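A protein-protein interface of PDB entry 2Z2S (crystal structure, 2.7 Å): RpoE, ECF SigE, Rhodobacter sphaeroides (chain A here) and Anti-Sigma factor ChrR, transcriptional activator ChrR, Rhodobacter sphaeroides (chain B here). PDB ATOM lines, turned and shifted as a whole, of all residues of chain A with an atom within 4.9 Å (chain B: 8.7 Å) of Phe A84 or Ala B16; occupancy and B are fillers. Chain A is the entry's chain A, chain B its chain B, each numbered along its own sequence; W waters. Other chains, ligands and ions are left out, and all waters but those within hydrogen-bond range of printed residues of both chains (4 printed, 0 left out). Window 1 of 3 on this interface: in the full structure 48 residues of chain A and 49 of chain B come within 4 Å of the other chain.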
ATOM      1  N   PHE A  43      10.529  -1.262  34.885  1.00  0.00           N
ATOM      2  CA  PHE A  43      10.061  -2.629  34.789  1.00  0.00           C
ATOM      3  C   PHE A  43      10.530  -3.443  35.991  1.00  0.00           C
ATOM      4  O   PHE A  43       9.719  -4.065  36.667  1.00  0.00           O
ATOM      5  CB  PHE A  43      10.592  -3.282  33.526  1.00  0.00           C
ATOM      6  CG  PHE A  43      10.110  -4.682  33.332  1.00  0.00           C
ATOM      7  CD1 PHE A  43       8.826  -4.927  32.861  1.00  0.00           C
ATOM      8  CD2 PHE A  43      10.934  -5.759  33.620  1.00  0.00           C
ATOM      9  CE1 PHE A  43       8.367  -6.213  32.673  1.00  0.00           C
ATOM     10  CE2 PHE A  43      10.479  -7.053  33.437  1.00  0.00           C
ATOM     11  CZ  PHE A  43       9.188  -7.277  32.958  1.00  0.00           C
ATOM     12  N   VAL A  79      13.439  -5.535  19.512  1.00  0.00           N
ATOM     13  CA  VAL A  79      14.575  -5.170  20.348  1.00  0.00           C
ATOM     14  C   VAL A  79      14.122  -5.101  21.793  1.00  0.00           C
ATOM     15  O   VAL A  79      14.857  -5.472  22.715  1.00  0.00           O
ATOM     16  CB  VAL A  79      15.168  -3.817  19.924  1.00  0.00           C
ATOM     17  CG1 VAL A  79      16.274  -3.416  20.882  1.00  0.00           C
ATOM     18  CG2 VAL A  79      15.707  -3.902  18.491  1.00  0.00           C
ATOM     19  N   ALA A  80      12.901  -4.632  21.996  1.00  0.00           N
ATOM     20  CA  ALA A  80      12.372  -4.567  23.349  1.00  0.00           C
ATOM     21  C   ALA A  80      12.207  -5.987  23.914  1.00  0.00           C
ATOM     22  O   ALA A  80      12.321  -6.196  25.119  1.00  0.00           O
ATOM     23  CB  ALA A  80      11.035  -3.831  23.367  1.00  0.00           C
ATOM     24  N   THR A  81      11.941  -6.967  23.058  1.00  0.00           N
ATOM     25  CA  THR A  81      11.796  -8.324  23.570  1.00  0.00           C
ATOM     26  C   THR A  81      13.155  -8.886  23.918  1.00  0.00           C
ATOM     27  O   THR A  81      13.328  -9.559  24.927  1.00  0.00           O
ATOM     28  CB  THR A  81      11.108  -9.264  22.567  1.00  0.00           C
ATOM     29  OG1 THR A  81       9.683  -9.062  22.628  1.00  0.00           O
ATOM     30  CG2 THR A  81      11.448 -10.726  22.875  1.00  0.00           C
ATOM     31  N   TRP A  82      14.130  -8.593  23.084  1.00  0.00           N
ATOM     32  CA  TRP A  82      15.472  -9.065  23.331  1.00  0.00           C
ATOM     33  C   TRP A  82      15.971  -8.456  24.650  1.00  0.00           C
ATOM     34  O   TRP A  82      16.505  -9.156  25.521  1.00  0.00           O
ATOM     35  CB  TRP A  82      16.375  -8.650  22.173  1.00  0.00           C
ATOM     36  CG  TRP A  82      17.721  -9.179  22.289  1.00  0.00           C
ATOM     37  CD1 TRP A  82      18.067 -10.484  22.338  1.00  0.00           C
ATOM     38  CD2 TRP A  82      18.940  -8.429  22.319  1.00  0.00           C
ATOM     39  NE1 TRP A  82      19.424 -10.605  22.392  1.00  0.00           N
ATOM     40  CE2 TRP A  82      19.992  -9.359  22.380  1.00  0.00           C
ATOM     41  CE3 TRP A  82      19.244  -7.057  22.299  1.00  0.00           C
ATOM     42  CZ2 TRP A  82      21.346  -8.977  22.418  1.00  0.00           C
ATOM     43  CZ3 TRP A  82      20.596  -6.667  22.340  1.00  0.00           C
ATOM     44  CH2 TRP A  82      21.628  -7.633  22.399  1.00  0.00           C
ATOM     45  N   ILE A  83      15.787  -7.150  24.796  1.00  0.00           N
ATOM     46  CA  ILE A  83      16.225  -6.484  25.995  1.00  0.00           C
ATOM     47  C   ILE A  83      15.503  -7.102  27.207  1.00  0.00           C
ATOM     48  O   ILE A  83      16.143  -7.360  28.234  1.00  0.00           O
ATOM     49  CB  ILE A  83      15.983  -4.958  25.869  1.00  0.00           C
ATOM     50  CG1 ILE A  83      17.050  -4.358  24.959  1.00  0.00           C
ATOM     51  CG2 ILE A  83      15.968  -4.281  27.239  1.00  0.00           C
ATOM     52  CD1 ILE A  83      16.908  -2.856  24.734  1.00  0.00           C
ATOM     53  N   PHE A  84      14.198  -7.369  27.085  1.00  0.00           N
ATOM     54  CA  PHE A  84      13.444  -7.979  28.181  1.00  0.00           C
ATOM     55  C   PHE A  84      14.128  -9.295  28.525  1.00  0.00           C
ATOM     56  O   PHE A  84      14.287  -9.650  29.686  1.00  0.00           O
ATOM     57  CB  PHE A  84      11.982  -8.240  27.777  1.00  0.00           C
ATOM     58  CG  PHE A  84      11.273  -9.208  28.680  1.00  0.00           C
ATOM     59  CD1 PHE A  84      11.156  -8.956  30.043  1.00  0.00           C
ATOM     60  CD2 PHE A  84      10.803 -10.415  28.186  1.00  0.00           C
ATOM     61  CE1 PHE A  84      10.592  -9.897  30.895  1.00  0.00           C
ATOM     62  CE2 PHE A  84      10.239 -11.356  29.023  1.00  0.00           C
ATOM     63  CZ  PHE A  84      10.134 -11.102  30.375  1.00  0.00           C
ATOM     64  N   THR A  85      14.554 -10.000  27.490  1.00  0.00           N
ATOM     65  CA  THR A  85      15.245 -11.262  27.648  1.00  0.00           C
ATOM     66  C   THR A  85      16.481 -11.128  28.515  1.00  0.00           C
ATOM     67  O   THR A  85      16.771 -12.012  29.319  1.00  0.00           O
ATOM     68  CB  THR A  85      15.647 -11.807  26.277  1.00  0.00           C
ATOM     69  OG1 THR A  85      14.516 -12.453  25.690  1.00  0.00           O
ATOM     70  CG2 THR A  85      16.821 -12.780  26.387  1.00  0.00           C
ATOM     71  N   ILE A  86      17.210 -10.024  28.351  1.00  0.00           N
ATOM     72  CA  ILE A  86      18.435  -9.786  29.123  1.00  0.00           C
ATOM     73  C   ILE A  86      18.164  -9.290  30.548  1.00  0.00           C
ATOM     74  O   ILE A  86      18.974  -9.471  31.455  1.00  0.00           O
ATOM     75  CB  ILE A  86      19.341  -8.782  28.394  1.00  0.00           C
ATOM     76  CG1 ILE A  86      19.734  -9.366  27.040  1.00  0.00           C
ATOM     77  CG2 ILE A  86      20.570  -8.481  29.233  1.00  0.00           C
ATOM     78  CD1 ILE A  86      20.552  -8.447  26.140  1.00  0.00           C
ATOM     79  N   ALA A  87      17.012  -8.669  30.737  1.00  0.00           N
ATOM     80  CA  ALA A  87      16.652  -8.166  32.043  1.00  0.00           C
ATOM     81  C   ALA A  87      16.222  -9.322  32.948  1.00  0.00           C
ATOM     82  O   ALA A  87      16.627  -9.420  34.108  1.00  0.00           O
ATOM     83  CB  ALA A  87      15.533  -7.162  31.913  1.00  0.00           C
ATOM     84  N   ARG A  88      15.410 -10.219  32.407  1.00  0.00           N
ATOM     85  CA  ARG A  88      14.929 -11.335  33.202  1.00  0.00           C
ATOM     86  C   ARG A  88      15.987 -12.395  33.499  1.00  0.00           C
ATOM     87  O   ARG A  88      15.885 -13.099  34.498  1.00  0.00           O
ATOM     88  CB  ARG A  88      13.702 -11.969  32.529  1.00  0.00           C
ATOM     89  CG  ARG A  88      13.962 -12.646  31.195  1.00  0.00           C
ATOM     90  CD  ARG A  88      14.061 -14.147  31.354  1.00  0.00           C
ATOM     91  NE  ARG A  88      14.344 -14.807  30.085  1.00  0.00           N
ATOM     92  CZ  ARG A  88      13.443 -15.041  29.134  1.00  0.00           C
ATOM     93  NH1 ARG A  88      12.178 -14.673  29.295  1.00  0.00           N
ATOM     94  NH2 ARG A  88      13.807 -15.654  28.015  1.00  0.00           N
ATOM     95  N   PHE A 148       4.432 -12.136  34.849  1.00  0.00           N
ATOM     96  CA  PHE A 148       5.754 -11.575  34.582  1.00  0.00           C
ATOM     97  C   PHE A 148       6.309 -10.741  35.723  1.00  0.00           C
ATOM     98  O   PHE A 148       7.369 -10.137  35.591  1.00  0.00           O
ATOM     99  CB  PHE A 148       5.748 -10.715  33.302  1.00  0.00           C
ATOM    100  CG  PHE A 148       5.686 -11.514  32.038  1.00  0.00           C
ATOM    101  CD1 PHE A 148       4.473 -11.854  31.473  1.00  0.00           C
ATOM    102  CD2 PHE A 148       6.851 -11.991  31.458  1.00  0.00           C
ATOM    103  CE1 PHE A 148       4.423 -12.662  30.356  1.00  0.00           C
ATOM    104  CE2 PHE A 148       6.808 -12.800  30.340  1.00  0.00           C
ATOM    105  CZ  PHE A 148       5.595 -13.137  29.791  1.00  0.00           C
ATOM    106  N   ASP B   9       3.057 -25.432  28.716  1.00  0.00           N
ATOM    107  CA  ASP B   9       2.931 -23.998  28.545  1.00  0.00           C
ATOM    108  C   ASP B   9       3.196 -23.265  29.842  1.00  0.00           C
ATOM    109  O   ASP B   9       3.755 -22.170  29.823  1.00  0.00           O
ATOM    110  CB  ASP B   9       1.541 -23.632  28.015  1.00  0.00           C
ATOM    111  CG  ASP B   9       1.315 -24.108  26.579  1.00  0.00           C
ATOM    112  OD1 ASP B   9       2.285 -24.069  25.790  1.00  0.00           O
ATOM    113  OD2 ASP B   9       0.169 -24.498  26.237  1.00  0.00           O
ATOM    114  N   ALA B  10       2.807 -23.879  30.962  1.00  0.00           N
ATOM    115  CA  ALA B  10       2.991 -23.283  32.285  1.00  0.00           C
ATOM    116  C   ALA B  10       4.472 -23.217  32.667  1.00  0.00           C
ATOM    117  O   ALA B  10       4.921 -22.289  33.344  1.00  0.00           O
ATOM    118  CB  ALA B  10       2.225 -24.056  33.299  1.00  0.00           C
ATOM    119  N   LEU B  11       5.245 -24.196  32.237  1.00  0.00           N
ATOM    120  CA  LEU B  11       6.662 -24.153  32.539  1.00  0.00           C
ATOM    121  C   LEU B  11       7.376 -23.165  31.608  1.00  0.00           C
ATOM    122  O   LEU B  11       8.379 -22.548  31.985  1.00  0.00           O
ATOM    123  CB  LEU B  11       7.278 -25.539  32.393  1.00  0.00           C
ATOM    124  CG  LEU B  11       7.157 -26.476  33.585  1.00  0.00           C
ATOM    125  CD1 LEU B  11       8.021 -27.697  33.338  1.00  0.00           C
ATOM    126  CD2 LEU B  11       7.604 -25.751  34.823  1.00  0.00           C
ATOM    127  N   LEU B  12       6.867 -23.025  30.390  1.00  0.00           N
ATOM    128  CA  LEU B  12       7.439 -22.099  29.427  1.00  0.00           C
ATOM    129  C   LEU B  12       7.145 -20.665  29.851  1.00  0.00           C
ATOM    130  O   LEU B  12       7.964 -19.772  29.651  1.00  0.00           O
ATOM    131  CB  LEU B  12       6.867 -22.370  28.046  1.00  0.00           C
ATOM    132  CG  LEU B  12       7.842 -23.024  27.067  1.00  0.00           C
ATOM    133  CD1 LEU B  12       8.758 -24.040  27.726  1.00  0.00           C
ATOM    134  CD2 LEU B  12       7.025 -23.664  26.006  1.00  0.00           C
ATOM    135  N   THR B  13       5.972 -20.441  30.434  1.00  0.00           N
ATOM    136  CA  THR B  13       5.628 -19.109  30.928  1.00  0.00           C
ATOM    137  C   THR B  13       6.520 -18.748  32.131  1.00  0.00           C
ATOM    138  O   THR B  13       6.956 -17.597  32.280  1.00  0.00           O
ATOM    139  CB  THR B  13       4.159 -19.027  31.361  1.00  0.00           C
ATOM    140  OG1 THR B  13       3.325 -19.291  30.231  1.00  0.00           O
ATOM    141  CG2 THR B  13       3.834 -17.639  31.893  1.00  0.00           C
ATOM    142  N   ALA B  14       6.782 -19.733  32.984  1.00  0.00           N
ATOM    143  CA  ALA B  14       7.632 -19.498  34.141  1.00  0.00           C
ATOM    144  C   ALA B  14       9.047 -19.215  33.668  1.00  0.00           C
ATOM    145  O   ALA B  14       9.695 -18.302  34.176  1.00  0.00           O
ATOM    146  CB  ALA B  14       7.633 -20.700  35.067  1.00  0.00           C
ATOM    147  N   TYR B  15       9.535 -19.993  32.702  1.00  0.00           N
ATOM    148  CA  TYR B  15      10.888 -19.769  32.189  1.00  0.00           C
ATOM    149  C   TYR B  15      11.000 -18.378  31.561  1.00  0.00           C
ATOM    150  O   TYR B  15      11.994 -17.684  31.741  1.00  0.00           O
ATOM    151  CB  TYR B  15      11.265 -20.821  31.140  1.00  0.00           C
ATOM    152  CG  TYR B  15      12.624 -20.581  30.510  1.00  0.00           C
ATOM    153  CD1 TYR B  15      13.791 -21.102  31.080  1.00  0.00           C
ATOM    154  CD2 TYR B  15      12.748 -19.792  29.369  1.00  0.00           C
ATOM    155  CE1 TYR B  15      15.059 -20.836  30.521  1.00  0.00           C
ATOM    156  CE2 TYR B  15      14.000 -19.515  28.801  1.00  0.00           C
ATOM    157  CZ  TYR B  15      15.155 -20.035  29.374  1.00  0.00           C
ATOM    158  OH  TYR B  15      16.388 -19.744  28.799  1.00  0.00           O
ATOM    159  N   ALA B  16       9.973 -17.986  30.809  1.00  0.00           N
ATOM    160  CA  ALA B  16       9.955 -16.676  30.162  1.00  0.00           C
ATOM    161  C   ALA B  16       9.832 -15.558  31.205  1.00  0.00           C
ATOM    162  O   ALA B  16      10.279 -14.436  30.978  1.00  0.00           O
ATOM    163  CB  ALA B  16       8.801 -16.598  29.154  1.00  0.00           C
ATOM    164  N   ALA B  17       9.220 -15.857  32.346  1.00  0.00           N
ATOM    165  CA  ALA B  17       9.081 -14.852  33.396  1.00  0.00           C
ATOM    166  C   ALA B  17      10.395 -14.809  34.194  1.00  0.00           C
ATOM    167  O   ALA B  17      10.733 -13.810  34.824  1.00  0.00           O
ATOM    168  CB  ALA B  17       7.908 -15.203  34.307  1.00  0.00           C
ATOM    169  N   GLY B  18      11.142 -15.904  34.137  1.00  0.00           N
ATOM    170  CA  GLY B  18      12.400 -15.978  34.852  1.00  0.00           C
ATOM    171  C   GLY B  18      12.217 -16.312  36.317  1.00  0.00           C
ATOM    172  O   GLY B  18      13.156 -16.168  37.106  1.00  0.00           O
ATOM    173  N   THR B  19      11.023 -16.770  36.684  1.00  0.00           N
ATOM    174  CA  THR B  19      10.736 -17.102  38.073  1.00  0.00           C
ATOM    175  C   THR B  19      11.091 -18.547  38.435  1.00  0.00           C
ATOM    176  O   THR B  19      10.882 -18.987  39.563  1.00  0.00           O
ATOM    177  CB  THR B  19       9.255 -16.886  38.370  1.00  0.00           C
ATOM    178  OG1 THR B  19       8.485 -17.879  37.685  1.00  0.00           O
ATOM    179  CG2 THR B  19       8.826 -15.506  37.905  1.00  0.00           C
ATOM    180  N   LEU B  20      11.641 -19.272  37.473  1.00  0.00           N
ATOM    181  CA  LEU B  20      11.994 -20.673  37.654  1.00  0.00           C
ATOM    182  C   LEU B  20      13.260 -20.845  38.460  1.00  0.00           C
ATOM    183  O   LEU B  20      14.134 -19.975  38.435  1.00  0.00           O
ATOM    184  CB  LEU B  20      12.162 -21.318  36.279  1.00  0.00           C
ATOM    185  CG  LEU B  20      11.345 -22.571  35.988  1.00  0.00           C
ATOM    186  CD1 LEU B  20       9.895 -22.374  36.411  1.00  0.00           C
ATOM    187  CD2 LEU B  20      11.440 -22.879  34.514  1.00  0.00           C
ATOM    188  N   SER B  25      15.170 -24.500  35.300  1.00  0.00           N
ATOM    189  CA  SER B  25      15.615 -23.674  34.182  1.00  0.00           C
ATOM    190  C   SER B  25      16.647 -24.434  33.371  1.00  0.00           C
ATOM    191  O   SER B  25      16.745 -24.275  32.164  1.00  0.00           O
ATOM    192  CB  SER B  25      16.256 -22.388  34.683  1.00  0.00           C
ATOM    193  OG  SER B  25      15.339 -21.636  35.455  1.00  0.00           O
ATOM    194  N   VAL B  28      14.573 -27.155  31.262  1.00  0.00           N
ATOM    195  CA  VAL B  28      13.747 -26.490  30.273  1.00  0.00           C
ATOM    196  C   VAL B  28      14.586 -25.909  29.139  1.00  0.00           C
ATOM    197  O   VAL B  28      14.266 -26.082  27.962  1.00  0.00           O
ATOM    198  CB  VAL B  28      12.931 -25.379  30.905  1.00  0.00           C
ATOM    199  CG1 VAL B  28      12.177 -24.620  29.839  1.00  0.00           C
ATOM    200  CG2 VAL B  28      11.965 -25.971  31.886  1.00  0.00           C
ATOM    201  N   LEU B  32      14.948 -26.610  25.153  1.00  0.00           N
ATOM    202  CA  LEU B  32      14.850 -25.505  24.205  1.00  0.00           C
ATOM    203  C   LEU B  32      15.976 -25.481  23.191  1.00  0.00           C
ATOM    204  O   LEU B  32      15.769 -25.102  22.037  1.00  0.00           O
ATOM    205  CB  LEU B  32      14.790 -24.142  24.916  1.00  0.00           C
ATOM    206  CG  LEU B  32      13.546 -23.755  25.736  1.00  0.00           C
ATOM    207  CD1 LEU B  32      13.601 -22.281  26.050  1.00  0.00           C
ATOM    208  CD2 LEU B  32      12.270 -24.067  24.983  1.00  0.00           C
ATOM    209  N   ARG B  41       8.044 -21.337  20.930  1.00  0.00           N
ATOM    210  CA  ARG B  41       7.019 -21.056  21.933  1.00  0.00           C
ATOM    211  C   ARG B  41       7.537 -20.071  22.990  1.00  0.00           C
ATOM    212  O   ARG B  41       6.850 -19.099  23.343  1.00  0.00           O
ATOM    213  CB  ARG B  41       6.588 -22.339  22.609  1.00  0.00           C
ATOM    214  CG  ARG B  41       6.040 -23.337  21.648  1.00  0.00           C
ATOM    215  CD  ARG B  41       5.383 -24.434  22.429  1.00  0.00           C
ATOM    216  NE  ARG B  41       5.015 -25.572  21.602  1.00  0.00           N
ATOM    217  CZ  ARG B  41       4.571 -26.726  22.081  1.00  0.00           C
ATOM    218  NH1 ARG B  41       4.429 -26.890  23.395  1.00  0.00           N
ATOM    219  NH2 ARG B  41       4.326 -27.731  21.247  1.00  0.00           N
ATOM    220  N   ALA B  42       8.751 -20.324  23.487  1.00  0.00           N
ATOM    221  CA  ALA B  42       9.352 -19.438  24.470  1.00  0.00           C
ATOM    222  C   ALA B  42       9.400 -18.036  23.854  1.00  0.00           C
ATOM    223  O   ALA B  42       9.043 -17.030  24.482  1.00  0.00           O
ATOM    224  CB  ALA B  42      10.754 -19.907  24.807  1.00  0.00           C
ATOM    225  N   GLY B  43       9.827 -17.981  22.600  1.00  0.00           N
ATOM    226  CA  GLY B  43       9.904 -16.712  21.922  1.00  0.00           C
ATOM    227  C   GLY B  43       8.607 -15.933  21.936  1.00  0.00           C
ATOM    228  O   GLY B  43       8.618 -14.732  22.201  1.00  0.00           O
ATOM    229  N   ALA B  44       7.486 -16.582  21.632  1.00  0.00           N
ATOM    230  CA  ALA B  44       6.226 -15.854  21.645  1.00  0.00           C
ATOM    231  C   ALA B  44       5.985 -15.334  23.062  1.00  0.00           C
ATOM    232  O   ALA B  44       5.573 -14.189  23.272  1.00  0.00           O
ATOM    233  CB  ALA B  44       5.104 -16.754  21.229  1.00  0.00           C
ATOM    234  N   LEU B  45       6.259 -16.190  24.041  1.00  0.00           N
ATOM    235  CA  LEU B  45       6.099 -15.803  25.435  1.00  0.00           C
ATOM    236  C   LEU B  45       7.028 -14.644  25.802  1.00  0.00           C
ATOM    237  O   LEU B  45       6.622 -13.750  26.545  1.00  0.00           O
ATOM    238  CB  LEU B  45       6.342 -17.002  26.351  1.00  0.00           C
ATOM    239  CG  LEU B  45       5.124 -17.620  27.053  1.00  0.00           C
ATOM    240  CD1 LEU B  45       3.809 -17.113  26.466  1.00  0.00           C
ATOM    241  CD2 LEU B  45       5.229 -19.127  26.947  1.00  0.00           C
ATOM    242  N   ASP B  46       8.256 -14.648  25.279  1.00  0.00           N
ATOM    243  CA  ASP B  46       9.184 -13.549  25.563  1.00  0.00           C
ATOM    244  C   ASP B  46       8.580 -12.271  24.970  1.00  0.00           C
ATOM    245  O   ASP B  46       8.742 -11.185  25.518  1.00  0.00           O
ATOM    246  CB  ASP B  46      10.576 -13.775  24.924  1.00  0.00           C
ATOM    247  CG  ASP B  46      11.282 -15.040  25.424  1.00  0.00           C
ATOM    248  OD1 ASP B  46      11.455 -15.221  26.660  1.00  0.00           O
ATOM    249  OD2 ASP B  46      11.680 -15.856  24.560  1.00  0.00           O
ATOM    250  N   ALA B  47       7.874 -12.416  23.848  1.00  0.00           N
ATOM    251  CA  ALA B  47       7.271 -11.271  23.178  1.00  0.00           C
ATOM    252  C   ALA B  47       6.266 -10.580  24.071  1.00  0.00           C
ATOM    253  O   ALA B  47       6.087  -9.362  23.991  1.00  0.00           O
ATOM    254  CB  ALA B  47       6.603 -11.704  21.896  1.00  0.00           C
ATOM    255  N   VAL B  48       5.590 -11.355  24.912  1.00  0.00           N
ATOM    256  CA  VAL B  48       4.629 -10.762  25.831  1.00  0.00           C
ATOM    257  C   VAL B  48       5.410  -9.870  26.800  1.00  0.00           C
ATOM    258  O   VAL B  48       5.006  -8.741  27.092  1.00  0.00           O
ATOM    259  CB  VAL B  48       3.862 -11.840  26.624  1.00  0.00           C
ATOM    260  CG1 VAL B  48       2.934 -11.186  27.617  1.00  0.00           C
ATOM    261  CG2 VAL B  48       3.061 -12.706  25.670  1.00  0.00           C
ATOM    262  N   GLY B  49       6.543 -10.387  27.271  1.00  0.00           N
ATOM    263  CA  GLY B  49       7.383  -9.641  28.189  1.00  0.00           C
ATOM    264  C   GLY B  49       7.929  -8.371  27.564  1.00  0.00           C
ATOM    265  O   GLY B  49       7.942  -7.319  28.199  1.00  0.00           O
ATOM    266  N   GLY B  50       8.381  -8.462  26.316  1.00  0.00           N
ATOM    267  CA  GLY B  50       8.920  -7.295  25.645  1.00  0.00           C
ATOM    268  C   GLY B  50       7.871  -6.223  25.470  1.00  0.00           C
ATOM    269  O   GLY B  50       8.190  -5.037  25.465  1.00  0.00           O
ATOM    270  N   SER B  51       6.616  -6.637  25.314  1.00  0.00           N
ATOM    271  CA  SER B  51       5.541  -5.682  25.144  1.00  0.00           C
ATOM    272  C   SER B  51       5.219  -5.003  26.461  1.00  0.00           C
ATOM    273  O   SER B  51       5.084  -3.783  26.506  1.00  0.00           O
ATOM    274  CB  SER B  51       4.316  -6.373  24.581  1.00  0.00           C
ATOM    275  OG  SER B  51       4.551  -6.727  23.232  1.00  0.00           O
ATOM    276  N   LEU B  52       5.096  -5.780  27.533  1.00  0.00           N
ATOM    277  CA  LEU B  52       4.829  -5.199  28.851  1.00  0.00           C
ATOM    278  C   LEU B  52       5.979  -4.236  29.136  1.00  0.00           C
ATOM    279  O   LEU B  52       5.800  -3.165  29.706  1.00  0.00           O
ATOM    280  CB  LEU B  52       4.798  -6.287  29.932  1.00  0.00           C
ATOM    281  CG  LEU B  52       3.618  -7.248  29.905  1.00  0.00           C
ATOM    282  CD1 LEU B  52       3.814  -8.382  30.900  1.00  0.00           C
ATOM    283  CD2 LEU B  52       2.373  -6.452  30.224  1.00  0.00           C
ATOM    284  N   MET B  53       7.165  -4.650  28.719  1.00  0.00           N
ATOM    285  CA  MET B  53       8.378  -3.877  28.881  1.00  0.00           C
ATOM    286  C   MET B  53       8.221  -2.497  28.275  1.00  0.00           C
ATOM    287  O   MET B  53       8.348  -1.474  28.945  1.00  0.00           O
ATOM    288  CB  MET B  53       9.511  -4.606  28.171  1.00  0.00           C
ATOM    289  CG  MET B  53      10.755  -3.789  27.905  1.00  0.00           C
ATOM    290  SD  MET B  53      11.772  -3.543  29.499  1.00  0.00           S
ATOM    291  CE  MET B  53      12.526  -5.339  29.704  1.00  0.00           C
ATOM    292  N   GLU B  54       7.945  -2.498  26.979  1.00  0.00           N
ATOM    293  CA  GLU B  54       7.787  -1.293  26.196  1.00  0.00           C
ATOM    294  C   GLU B  54       6.638  -0.413  26.656  1.00  0.00           C
ATOM    295  O   GLU B  54       6.676   0.794  26.451  1.00  0.00           O
ATOM    296  CB  GLU B  54       7.611  -1.686  24.730  1.00  0.00           C
ATOM    297  CG  GLU B  54       7.326  -0.536  23.796  1.00  0.00           C
ATOM    298  CD  GLU B  54       8.435   0.498  23.780  1.00  0.00           C
ATOM    299  OE1 GLU B  54       9.580   0.132  23.421  1.00  0.00           O
ATOM    300  OE2 GLU B  54       8.147   1.671  24.122  1.00  0.00           O
HETATM  301  O   HOH W   1      16.916 -16.979  28.302  1.00  0.00           O
HETATM  302  O   HOH W   2       7.200  -7.134  21.925  1.00  0.00           O
HETATM  303  O   HOH W   3      14.057 -16.891  25.007  1.00  0.00           O
HETATM  304  O   HOH W   4       9.093 -11.465  34.143  1.00  0.00           O
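NH1 of Arg A88 is in hydrogen-bond range of O of Ala B16, 2.5 Å away. NH2 of Arg A88 is in salt-bridge range of OD1 of Asp B46.
The backbone carbonyl oxygen (O) of Thr A81 sits at hydrogen-bond distance from the side-chain hydroxyl (OG1) of Thr A85 (3.2 Å). OD2 of Asp B46 lies close to N of Gly B43, at 3.4 Å. The backbone carbonyl oxygen (O) of Ala B47 sits at hydrogen-bond distance from the side-chain hydroxyl (OG) of Ser B51, at 3.1 Å.
Among the printed residues, pairs that only touch across the chains: Phe A84 with Met B53, Thr A81 with Ala B47, Phe A84 with Ala B16, Phe A84 with Gly B49, Phe A148 with Val B48, Phe A84 with Asp B46, Phe A148 with Leu B45, Thr A81 with Gly B50, Phe A148 with Leu B52, Ala A80 with Gly B50, Phe A84 with Gly B50, Thr A81 with Asp B46, Phe A148 with Gly B49, Arg A88 with Tyr B15 and Phe A148 with Ala B16.
Of chain B, only Ala B16 (3.4 Å), Asp B46 (3.5 Å), Gly B49 (3.4 Å), Gly B50 (3.6 Å) and Met B53 (3.2 Å) come within 4 Å of Phe A84. Ala B16 touches just these residues of chain A: Phe A84 (3.4 Å), Arg A88 (2.5 Å) and Phe A148 (3.9 Å). Printed residues of chain A within 4 Å of Leu B45: Phe A148 (3.5 Å). Of the printed residues of chain B, Ala A80 touches Gly B50. Of the printed residues of chain B, Phe A148 touches Ala B16 (3.9 Å), Leu B45 (3.5 Å), Val B48 (3.4 Å), Gly B49 (3.8 Å) and Leu B52 (3.6 Å). Printed residues of chain A within 4 Å of Val B48: Phe A148. Printed residues of chain A within 4 Å of Met B53: Phe A84 (3.2 Å). Val A79 touches none of the printed residues of chain B. Ser B25 touches none of the printed residues of chain A. The nearest residue of chain B that does not touch Phe A84 is Ala B17 (4.9 Å). The nearest printed residue of chain A that does not touch Ala B16 is Thr A85 (6.8 Å).
Hydrophobic or aromatic side chains of chain B within 4 Å of the printed part of chain A: Tyr B15, Ala B16, Val B48, Leu B52 and Met B53. Of the 12 printed residues of chain A, 5 touch a printed residue of chain B. Printed residues of chain A that touch a printed residue of chain B: Ala A80, Thr A81, Phe A84, Arg A88 and Phe A148. Hydrophobic or aromatic side chains of chain A within 4 Å of the printed part of chain B: Ala A80, Phe A84 and Phe A148. Among the printed residues, Asp or Glu carboxylates within 4 Å of a Lys or Arg side-chain nitrogen of the other chain: Arg A88 with Asp B46 (2.7 Å).
Water W4 lies within hydrogen-bond range of the backbone carbonyl oxygen (O) of Phe A148 (2.6 Å) and the backbone carbonyl oxygen (O) of Ala B17 (2.9 Å). Water W3 lies within hydrogen-bond range of the side-chain carboxylate (OD2) of Asp B46 (2.6 Å) and the guanidinium group (NH2) of Arg A88 (3.3 Å). Water W1 lies within hydrogen-bond range of OH of Tyr B15 (2.9 Å) and NH2 of Arg A88 (3.4 Å). Water W2 lies within hydrogen-bond range of OG of Ser B51, OG1 of Thr A81 and O of Ala B47.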
